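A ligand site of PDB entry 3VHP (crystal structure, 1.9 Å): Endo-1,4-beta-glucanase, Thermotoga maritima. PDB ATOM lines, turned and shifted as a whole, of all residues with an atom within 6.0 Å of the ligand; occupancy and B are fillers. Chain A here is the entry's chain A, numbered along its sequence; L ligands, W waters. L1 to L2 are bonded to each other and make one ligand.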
ATOM      1  N   GLU A  30      18.456 -13.763  34.209  1.00  0.00           N
ATOM      2  CA  GLU A  30      17.937 -13.482  32.875  1.00  0.00           C
ATOM      3  C   GLU A  30      16.420 -13.569  32.814  1.00  0.00           C
ATOM      4  O   GLU A  30      15.821 -14.632  33.062  1.00  0.00           O
ATOM      5  CB  GLU A  30      18.472 -14.451  31.787  1.00  0.00           C
ATOM      6  CG  GLU A  30      18.059 -13.998  30.343  1.00  0.00           C
ATOM      7  CD  GLU A  30      18.393 -15.015  29.216  1.00  0.00           C
ATOM      8  OE1 GLU A  30      19.335 -15.833  29.354  1.00  0.00           O
ATOM      9  OE2 GLU A  30      17.721 -14.972  28.166  1.00  0.00           O
ATOM     10  N   ASN A  32      14.334 -14.283  30.806  1.00  0.00           N
ATOM     11  CA  ASN A  32      14.359 -15.036  29.544  1.00  0.00           C
ATOM     12  C   ASN A  32      12.984 -15.388  28.944  1.00  0.00           C
ATOM     13  O   ASN A  32      12.313 -16.293  29.434  1.00  0.00           O
ATOM     14  CB  ASN A  32      15.139 -16.327  29.834  1.00  0.00           C
ATOM     15  CG  ASN A  32      15.281 -17.222  28.626  1.00  0.00           C
ATOM     16  OD1 ASN A  32      14.700 -16.967  27.575  1.00  0.00           O
ATOM     17  ND2 ASN A  32      16.077 -18.273  28.771  1.00  0.00           N
ATOM     18  N   TRP A  34      12.744 -16.167  25.677  1.00  0.00           N
ATOM     19  CA  TRP A  34      13.304 -16.435  24.337  1.00  0.00           C
ATOM     20  C   TRP A  34      12.352 -16.905  23.245  1.00  0.00           C
ATOM     21  O   TRP A  34      12.550 -16.588  22.087  1.00  0.00           O
ATOM     22  CB  TRP A  34      14.475 -17.445  24.428  1.00  0.00           C
ATOM     23  CG  TRP A  34      14.035 -18.837  24.759  1.00  0.00           C
ATOM     24  CD1 TRP A  34      13.725 -19.351  25.988  1.00  0.00           C
ATOM     25  CD2 TRP A  34      13.763 -19.858  23.819  1.00  0.00           C
ATOM     26  NE1 TRP A  34      13.258 -20.642  25.865  1.00  0.00           N
ATOM     27  CE2 TRP A  34      13.283 -20.978  24.541  1.00  0.00           C
ATOM     28  CE3 TRP A  34      13.880 -19.948  22.428  1.00  0.00           C
ATOM     29  CZ2 TRP A  34      12.913 -22.170  23.915  1.00  0.00           C
ATOM     30  CZ3 TRP A  34      13.514 -21.128  21.809  1.00  0.00           C
ATOM     31  CH2 TRP A  34      13.037 -22.217  22.548  1.00  0.00           C
ATOM     32  N   GLU A  65       9.305 -19.555  17.502  1.00  0.00           N
ATOM     33  CA  GLU A  65       9.555 -20.647  16.554  1.00  0.00           C
ATOM     34  C   GLU A  65       8.499 -21.689  16.856  1.00  0.00           C
ATOM     35  O   GLU A  65       8.687 -22.588  17.677  1.00  0.00           O
ATOM     36  CB  GLU A  65      10.973 -21.244  16.683  1.00  0.00           C
ATOM     37  CG  GLU A  65      11.536 -21.373  18.097  1.00  0.00           C
ATOM     38  CD  GLU A  65      11.677 -22.827  18.611  1.00  0.00           C
ATOM     39  OE1 GLU A  65      10.664 -23.386  19.101  1.00  0.00           O
ATOM     40  OE2 GLU A  65      12.797 -23.400  18.526  1.00  0.00           O
ATOM     41  N   VAL A  71       8.067 -25.084  25.158  1.00  0.00           N
ATOM     42  CA  VAL A  71       7.821 -23.864  25.925  1.00  0.00           C
ATOM     43  C   VAL A  71       8.141 -22.512  25.318  1.00  0.00           C
ATOM     44  O   VAL A  71       8.825 -22.383  24.316  1.00  0.00           O
ATOM     45  CB  VAL A  71       8.492 -23.959  27.337  1.00  0.00           C
ATOM     46  CG1 VAL A  71       8.353 -25.382  27.881  1.00  0.00           C
ATOM     47  CG2 VAL A  71       9.940 -23.575  27.262  1.00  0.00           C
ATOM     48  N   GLY A  73       9.177 -19.589  27.479  1.00  0.00           N
ATOM     49  CA  GLY A  73      10.236 -18.847  28.133  1.00  0.00           C
ATOM     50  C   GLY A  73      10.777 -19.567  29.326  1.00  0.00           C
ATOM     51  O   GLY A  73      10.282 -20.627  29.709  1.00  0.00           O
ATOM     52  N   TYR A  74      11.789 -18.974  29.925  1.00  0.00           N
ATOM     53  CA  TYR A  74      12.468 -19.596  31.041  1.00  0.00           C
ATOM     54  C   TYR A  74      13.142 -18.581  31.973  1.00  0.00           C
ATOM     55  O   TYR A  74      14.376 -18.511  32.016  1.00  0.00           O
ATOM     56  CB  TYR A  74      13.498 -20.589  30.441  1.00  0.00           C
ATOM     57  CG  TYR A  74      14.342 -21.401  31.429  1.00  0.00           C
ATOM     58  CD1 TYR A  74      13.758 -22.087  32.508  1.00  0.00           C
ATOM     59  CD2 TYR A  74      15.719 -21.521  31.229  1.00  0.00           C
ATOM     60  CE1 TYR A  74      14.570 -22.899  33.401  1.00  0.00           C
ATOM     61  CE2 TYR A  74      16.523 -22.307  32.098  1.00  0.00           C
ATOM     62  CZ  TYR A  74      15.950 -22.985  33.172  1.00  0.00           C
ATOM     63  OH  TYR A  74      16.749 -23.767  33.982  1.00  0.00           O
ATOM     64  N   GLU A  76      15.066 -17.127  34.739  1.00  0.00           N
ATOM     65  CA  GLU A  76      16.070 -17.900  35.453  1.00  0.00           C
ATOM     66  C   GLU A  76      17.214 -17.061  35.975  1.00  0.00           C
ATOM     67  O   GLU A  76      17.284 -15.863  35.705  1.00  0.00           O
ATOM     68  CB  GLU A  76      16.670 -18.831  34.396  1.00  0.00           C
ATOM     69  CG  GLU A  76      17.412 -17.983  33.292  1.00  0.00           C
ATOM     70  CD  GLU A  76      18.211 -18.819  32.309  1.00  0.00           C
ATOM     71  OE1 GLU A  76      19.081 -19.578  32.780  1.00  0.00           O
ATOM     72  OE2 GLU A  76      17.945 -18.758  31.099  1.00  0.00           O
ATOM     73  N   LYS A  82      26.632 -19.069  30.142  1.00  0.00           N
ATOM     74  CA  LYS A  82      25.510 -19.554  29.345  1.00  0.00           C
ATOM     75  C   LYS A  82      25.945 -19.352  27.899  1.00  0.00           C
ATOM     76  O   LYS A  82      26.046 -18.228  27.427  1.00  0.00           O
ATOM     77  CB  LYS A  82      24.245 -18.725  29.611  1.00  0.00           C
ATOM     78  CG  LYS A  82      23.062 -19.311  28.883  1.00  0.00           C
ATOM     79  CD  LYS A  82      21.776 -18.637  29.311  1.00  0.00           C
ATOM     80  CE  LYS A  82      20.649 -19.173  28.404  1.00  0.00           C
ATOM     81  NZ  LYS A  82      19.386 -18.489  28.763  1.00  0.00           N
ATOM     82  N   TRP A  84      24.491 -19.658  24.845  1.00  0.00           N
ATOM     83  CA  TRP A  84      23.601 -18.930  23.975  1.00  0.00           C
ATOM     84  C   TRP A  84      23.734 -17.412  24.076  1.00  0.00           C
ATOM     85  O   TRP A  84      23.457 -16.681  23.115  1.00  0.00           O
ATOM     86  CB  TRP A  84      22.175 -19.361  24.282  1.00  0.00           C
ATOM     87  CG  TRP A  84      21.960 -20.825  24.012  1.00  0.00           C
ATOM     88  CD1 TRP A  84      21.867 -21.851  24.948  1.00  0.00           C
ATOM     89  CD2 TRP A  84      21.779 -21.427  22.738  1.00  0.00           C
ATOM     90  NE1 TRP A  84      21.619 -23.041  24.297  1.00  0.00           N
ATOM     91  CE2 TRP A  84      21.558 -22.804  22.945  1.00  0.00           C
ATOM     92  CE3 TRP A  84      21.761 -20.916  21.410  1.00  0.00           C
ATOM     93  CZ2 TRP A  84      21.333 -23.684  21.893  1.00  0.00           C
ATOM     94  CZ3 TRP A  84      21.533 -21.800  20.366  1.00  0.00           C
ATOM     95  CH2 TRP A  84      21.327 -23.181  20.612  1.00  0.00           C
ATOM     96  N   GLU A  85      24.150 -16.935  25.245  1.00  0.00           N
ATOM     97  CA  GLU A  85      24.271 -15.499  25.442  1.00  0.00           C
ATOM     98  C   GLU A  85      25.725 -15.014  25.549  1.00  0.00           C
ATOM     99  O   GLU A  85      25.949 -13.823  25.768  1.00  0.00           O
ATOM    100  CB  GLU A  85      23.451 -15.086  26.700  1.00  0.00           C
ATOM    101  CG  GLU A  85      21.924 -15.295  26.563  1.00  0.00           C
ATOM    102  CD  GLU A  85      21.337 -14.388  25.482  1.00  0.00           C
ATOM    103  OE1 GLU A  85      21.861 -13.260  25.391  1.00  0.00           O
ATOM    104  OE2 GLU A  85      20.403 -14.763  24.727  1.00  0.00           O
ATOM    105  N   GLU A 125      19.196 -26.507  34.667  1.00  0.00           N
ATOM    106  CA  GLU A 125      19.869 -27.189  33.574  1.00  0.00           C
ATOM    107  C   GLU A 125      21.287 -26.706  33.313  1.00  0.00           C
ATOM    108  O   GLU A 125      21.730 -25.675  33.827  1.00  0.00           O
ATOM    109  CB  GLU A 125      19.073 -27.075  32.266  1.00  0.00           C
ATOM    110  CG  GLU A 125      19.014 -25.648  31.710  1.00  0.00           C
ATOM    111  CD  GLU A 125      18.372 -25.640  30.324  1.00  0.00           C
ATOM    112  OE1 GLU A 125      17.822 -24.599  29.912  1.00  0.00           O
ATOM    113  OE2 GLU A 125      18.409 -26.680  29.641  1.00  0.00           O
ATOM    114  N   TRP A 127      24.466 -26.982  29.991  1.00  0.00           N
ATOM    115  CA  TRP A 127      24.759 -27.195  28.580  1.00  0.00           C
ATOM    116  C   TRP A 127      26.184 -27.777  28.555  1.00  0.00           C
ATOM    117  O   TRP A 127      27.121 -27.110  29.045  1.00  0.00           O
ATOM    118  CB  TRP A 127      24.739 -25.860  27.816  1.00  0.00           C
ATOM    119  CG  TRP A 127      23.357 -25.248  27.742  1.00  0.00           C
ATOM    120  CD1 TRP A 127      22.785 -24.398  28.651  1.00  0.00           C
ATOM    121  CD2 TRP A 127      22.361 -25.526  26.753  1.00  0.00           C
ATOM    122  NE1 TRP A 127      21.485 -24.137  28.290  1.00  0.00           N
ATOM    123  CE2 TRP A 127      21.199 -24.816  27.128  1.00  0.00           C
ATOM    124  CE3 TRP A 127      22.333 -26.313  25.585  1.00  0.00           C
ATOM    125  CZ2 TRP A 127      20.008 -24.862  26.383  1.00  0.00           C
ATOM    126  CZ3 TRP A 127      21.159 -26.372  24.840  1.00  0.00           C
ATOM    127  CH2 TRP A 127      20.002 -25.643  25.237  1.00  0.00           C
ATOM    128  N   GLU A 143      22.184 -30.913  26.255  1.00  0.00           N
ATOM    129  CA  GLU A 143      21.403 -30.029  27.151  1.00  0.00           C
ATOM    130  C   GLU A 143      20.863 -31.038  28.213  1.00  0.00           C
ATOM    131  O   GLU A 143      20.197 -31.980  27.827  1.00  0.00           O
ATOM    132  CB  GLU A 143      20.230 -29.395  26.400  1.00  0.00           C
ATOM    133  CG  GLU A 143      19.469 -28.386  27.307  1.00  0.00           C
ATOM    134  CD  GLU A 143      18.165 -27.841  26.699  1.00  0.00           C
ATOM    135  OE1 GLU A 143      17.453 -27.115  27.424  1.00  0.00           O
ATOM    136  OE2 GLU A 143      17.860 -28.122  25.505  1.00  0.00           O
ATOM    137  N   MET A 145      18.604 -31.284  31.779  1.00  0.00           N
ATOM    138  CA  MET A 145      17.704 -30.592  32.711  1.00  0.00           C
ATOM    139  C   MET A 145      17.358 -31.479  33.906  1.00  0.00           C
ATOM    140  O   MET A 145      17.374 -32.720  33.809  1.00  0.00           O
ATOM    141  CB  MET A 145      16.415 -30.239  31.989  1.00  0.00           C
ATOM    142  CG  MET A 145      16.591 -29.613  30.624  1.00  0.00           C
ATOM    143  SD  MET A 145      15.068 -28.698  30.191  1.00  0.00           S
ATOM    144  CE  MET A 145      15.260 -27.243  31.225  1.00  0.00           C
ATOM    145  N   TRP A 185      17.531 -33.456  18.962  1.00  0.00           N
ATOM    146  CA  TRP A 185      17.123 -32.295  18.168  1.00  0.00           C
ATOM    147  C   TRP A 185      18.399 -31.709  17.554  1.00  0.00           C
ATOM    148  O   TRP A 185      19.213 -32.466  16.993  1.00  0.00           O
ATOM    149  CB  TRP A 185      16.421 -31.262  19.061  1.00  0.00           C
ATOM    150  CG  TRP A 185      15.110 -31.770  19.667  1.00  0.00           C
ATOM    151  CD1 TRP A 185      14.148 -32.563  19.045  1.00  0.00           C
ATOM    152  CD2 TRP A 185      14.544 -31.391  20.942  1.00  0.00           C
ATOM    153  NE1 TRP A 185      13.033 -32.678  19.860  1.00  0.00           N
ATOM    154  CE2 TRP A 185      13.250 -31.963  21.016  1.00  0.00           C
ATOM    155  CE3 TRP A 185      14.999 -30.604  22.009  1.00  0.00           C
ATOM    156  CZ2 TRP A 185      12.403 -31.778  22.126  1.00  0.00           C
ATOM    157  CZ3 TRP A 185      14.160 -30.416  23.124  1.00  0.00           C
ATOM    158  CH2 TRP A 185      12.877 -31.008  23.168  1.00  0.00           C
ATOM    159  N   TRP A 187      20.667 -30.657  19.115  1.00  0.00           N
ATOM    160  CA  TRP A 187      21.641 -31.129  20.097  1.00  0.00           C
ATOM    161  C   TRP A 187      20.920 -32.243  20.840  1.00  0.00           C
ATOM    162  O   TRP A 187      19.738 -32.495  20.562  1.00  0.00           O
ATOM    163  CB  TRP A 187      22.014 -30.004  21.067  1.00  0.00           C
ATOM    164  CG  TRP A 187      20.842 -29.304  21.727  1.00  0.00           C
ATOM    165  CD1 TRP A 187      20.190 -29.670  22.870  1.00  0.00           C
ATOM    166  CD2 TRP A 187      20.195 -28.111  21.261  1.00  0.00           C
ATOM    167  NE1 TRP A 187      19.162 -28.774  23.139  1.00  0.00           N
ATOM    168  CE2 TRP A 187      19.147 -27.818  22.164  1.00  0.00           C
ATOM    169  CE3 TRP A 187      20.391 -27.272  20.153  1.00  0.00           C
ATOM    170  CZ2 TRP A 187      18.300 -26.708  22.006  1.00  0.00           C
ATOM    171  CZ3 TRP A 187      19.549 -26.170  19.993  1.00  0.00           C
ATOM    172  CH2 TRP A 187      18.511 -25.899  20.911  1.00  0.00           C
ATOM    173  N   TYR A 189      19.039 -33.570  23.957  1.00  0.00           N
ATOM    174  CA  TYR A 189      18.296 -33.036  25.104  1.00  0.00           C
ATOM    175  C   TYR A 189      17.964 -34.168  26.087  1.00  0.00           C
ATOM    176  O   TYR A 189      17.360 -35.168  25.694  1.00  0.00           O
ATOM    177  CB  TYR A 189      17.002 -32.410  24.599  1.00  0.00           C
ATOM    178  CG  TYR A 189      15.919 -32.116  25.630  1.00  0.00           C
ATOM    179  CD1 TYR A 189      15.769 -30.831  26.158  1.00  0.00           C
ATOM    180  CD2 TYR A 189      14.981 -33.098  25.982  1.00  0.00           C
ATOM    181  CE1 TYR A 189      14.693 -30.519  26.989  1.00  0.00           C
ATOM    182  CE2 TYR A 189      13.906 -32.799  26.819  1.00  0.00           C
ATOM    183  CZ  TYR A 189      13.774 -31.506  27.311  1.00  0.00           C
ATOM    184  OH  TYR A 189      12.691 -31.184  28.061  1.00  0.00           O
ATOM    185  N   GLU A 236      21.823 -23.382  35.443  1.00  0.00           N
ATOM    186  CA  GLU A 236      20.697 -22.452  35.387  1.00  0.00           C
ATOM    187  C   GLU A 236      19.594 -22.970  36.276  1.00  0.00           C
ATOM    188  O   GLU A 236      19.381 -24.183  36.380  1.00  0.00           O
ATOM    189  CB  GLU A 236      20.173 -22.347  33.964  1.00  0.00           C
ATOM    190  CG  GLU A 236      21.249 -21.840  33.024  1.00  0.00           C
ATOM    191  CD  GLU A 236      20.782 -21.855  31.597  1.00  0.00           C
ATOM    192  OE1 GLU A 236      19.922 -21.024  31.213  1.00  0.00           O
ATOM    193  OE2 GLU A 236      21.281 -22.703  30.863  1.00  0.00           O
ATOM    194  N   GLU A 240      10.459 -23.030  33.376  1.00  0.00           N
ATOM    195  CA  GLU A 240      10.033 -23.010  31.981  1.00  0.00           C
ATOM    196  C   GLU A 240       8.494 -22.899  32.046  1.00  0.00           C
ATOM    197  O   GLU A 240       7.872 -23.377  32.991  1.00  0.00           O
ATOM    198  CB  GLU A 240      10.362 -24.314  31.250  1.00  0.00           C
ATOM    199  CG  GLU A 240      11.817 -24.574  31.067  1.00  0.00           C
ATOM    200  CD  GLU A 240      12.008 -25.747  30.128  1.00  0.00           C
ATOM    201  OE1 GLU A 240      11.637 -26.865  30.456  1.00  0.00           O
ATOM    202  OE2 GLU A 240      12.519 -25.530  29.035  1.00  0.00           O
HETATM  203  C1  LIG L   1      15.069 -26.064  24.917  1.00  0.00           C
HETATM  204  C2  LIG L   1      16.212 -25.054  25.066  1.00  0.00           C
HETATM  205  C3  LIG L   1      15.744 -23.857  25.904  1.00  0.00           C
HETATM  206  C4  LIG L   1      15.295 -24.422  27.245  1.00  0.00           C
HETATM  207  C5  LIG L   1      14.873 -23.322  28.216  1.00  0.00           C
HETATM  208  C6  LIG L   1      14.471 -26.423  26.283  1.00  0.00           C
HETATM  209  O1  LIG L   1      13.244 -27.134  26.087  1.00  0.00           O
HETATM  210  O2  LIG L   1      15.601 -27.256  24.329  1.00  0.00           O
HETATM  211  O3  LIG L   1      16.600 -24.618  23.767  1.00  0.00           O
HETATM  212  O4  LIG L   1      16.856 -22.989  26.159  1.00  0.00           O
HETATM  213  O5  LIG L   1      14.129 -25.227  27.002  1.00  0.00           O
HETATM  214  O6  LIG L   1      13.580 -22.859  27.819  1.00  0.00           O
HETATM  215  C1  LG2 L   2      17.837 -20.819  26.028  1.00  0.00           C
HETATM  216  C2  LG2 L   2      17.857 -19.525  25.199  1.00  0.00           C
HETATM  217  C3  LG2 L   2      18.277 -19.865  23.771  1.00  0.00           C
HETATM  218  C4  LG2 L   2      17.434 -21.005  23.185  1.00  0.00           C
HETATM  219  C5  LG2 L   2      17.998 -21.403  21.816  1.00  0.00           C
HETATM  220  C6  LG2 L   2      16.886 -21.812  25.346  1.00  0.00           C
HETATM  221  O1  LG2 L   2      17.421 -20.557  27.371  1.00  0.00           O
HETATM  222  O2  LG2 L   2      18.799 -18.603  25.748  1.00  0.00           O
HETATM  223  O3  LG2 L   2      18.070 -18.710  22.966  1.00  0.00           O
HETATM  224  O4  LG2 L   2      17.468 -22.135  24.069  1.00  0.00           O
HETATM  225  O5  LG2 L   2      17.198 -22.440  21.238  1.00  0.00           O
HETATM  226  O   HOH W   1      18.104 -16.104  25.917  1.00  0.00           O
HETATM  227  O   HOH W   2      11.712 -26.423  24.066  1.00  0.00           O
HETATM  228  O   HOH W   3      11.834 -28.554  28.131  1.00  0.00           O
HETATM  229  O   HOH W   4      18.614 -22.144  28.935  1.00  0.00           O
HETATM  230  O   HOH W   5      20.045 -16.638  23.010  1.00  0.00           O
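The side-chain amino group of Lys 82 is in hydrogen-bond range of an oxygen (O2) of LG2 L2. The side-chain carboxylate of Glu 240 is in hydrogen-bond range of an oxygen (O6) of LIG L1. The side-chain carboxylate (OE2) of Glu 143 sits at hydrogen-bond distance from an oxygen (O2) of LIG L1, at 2.7 Å. The indole nitrogen (NE1) of Trp 34 lies within hydrogen-bond range of an oxygen (O6) of LIG L1 (3.0 Å). O1 of LG2 L2 is in hydrogen-bond range of ND2 of Asn 32.
ND2 of Asn 32 is in hydrogen-bond range of OE2 of Glu 76, at 3.0 Å. The side-chain amide nitrogen (ND2) of Asn 32 sits close to the side-chain amino group (NZ) of Lys 82 (3.3 Å). The side-chain amino group (NZ) of Lys 82 lies within salt-bridge range of the side-chain carboxylate (OE1) of Glu 236. The side-chain amino group of Lys 82 lies within salt-bridge range of the side-chain carboxylate of Glu 76. N of Trp 34 is in hydrogen-bond range of OD1 of Asn 32. The side-chain carboxylate of Glu 143 sits at hydrogen-bond distance from the indole nitrogen of Trp 187. The side-chain carboxylate (OE2) of Glu 125 lies close to the side-chain carboxylate (OE1) of Glu 143 (2.5 Å). O of Glu 125 is in hydrogen-bond range of N of Glu 236 (2.8 Å).
Merely in contact with the ligand: Trp 187, Tyr 74, Glu 125, Trp 127, Trp 185, Val 71, Trp 84 and Tyr 189. Hydrophobic or aromatic side chains that line the ligand: Trp 34, Val 71, Tyr 74, Trp 84, Trp 127, Trp 185, Trp 187 and Tyr 189. Along chain A the residues within 4 Å of the ligand span positions 32 to 240.
Water W4 lies within hydrogen-bond range of O1 of LG2 L2 (2.5 Å), OE1 of Glu 125 (2.8 Å) and OE1 of Glu 236 (2.9 Å). Water W1 lies within hydrogen-bond range of OE2 of Glu 30 (2.5 Å), O2 of LG2 L2 (2.6 Å) and OE2 of Glu 85 (2.9 Å). Water W3 lies within hydrogen-bond range of OH of Tyr 189 (2.8 Å), O1 of LIG L1 (2.9 Å) and OE1 of Glu 240 (2.9 Å). Water W5 lies within hydrogen-bond range of the side-chain carboxylate of Glu 85 (2.6 Å), an oxygen (O3) of LG2 L2 (2.9 Å) and the backbone carbonyl oxygen of Trp 84 (3.4 Å).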
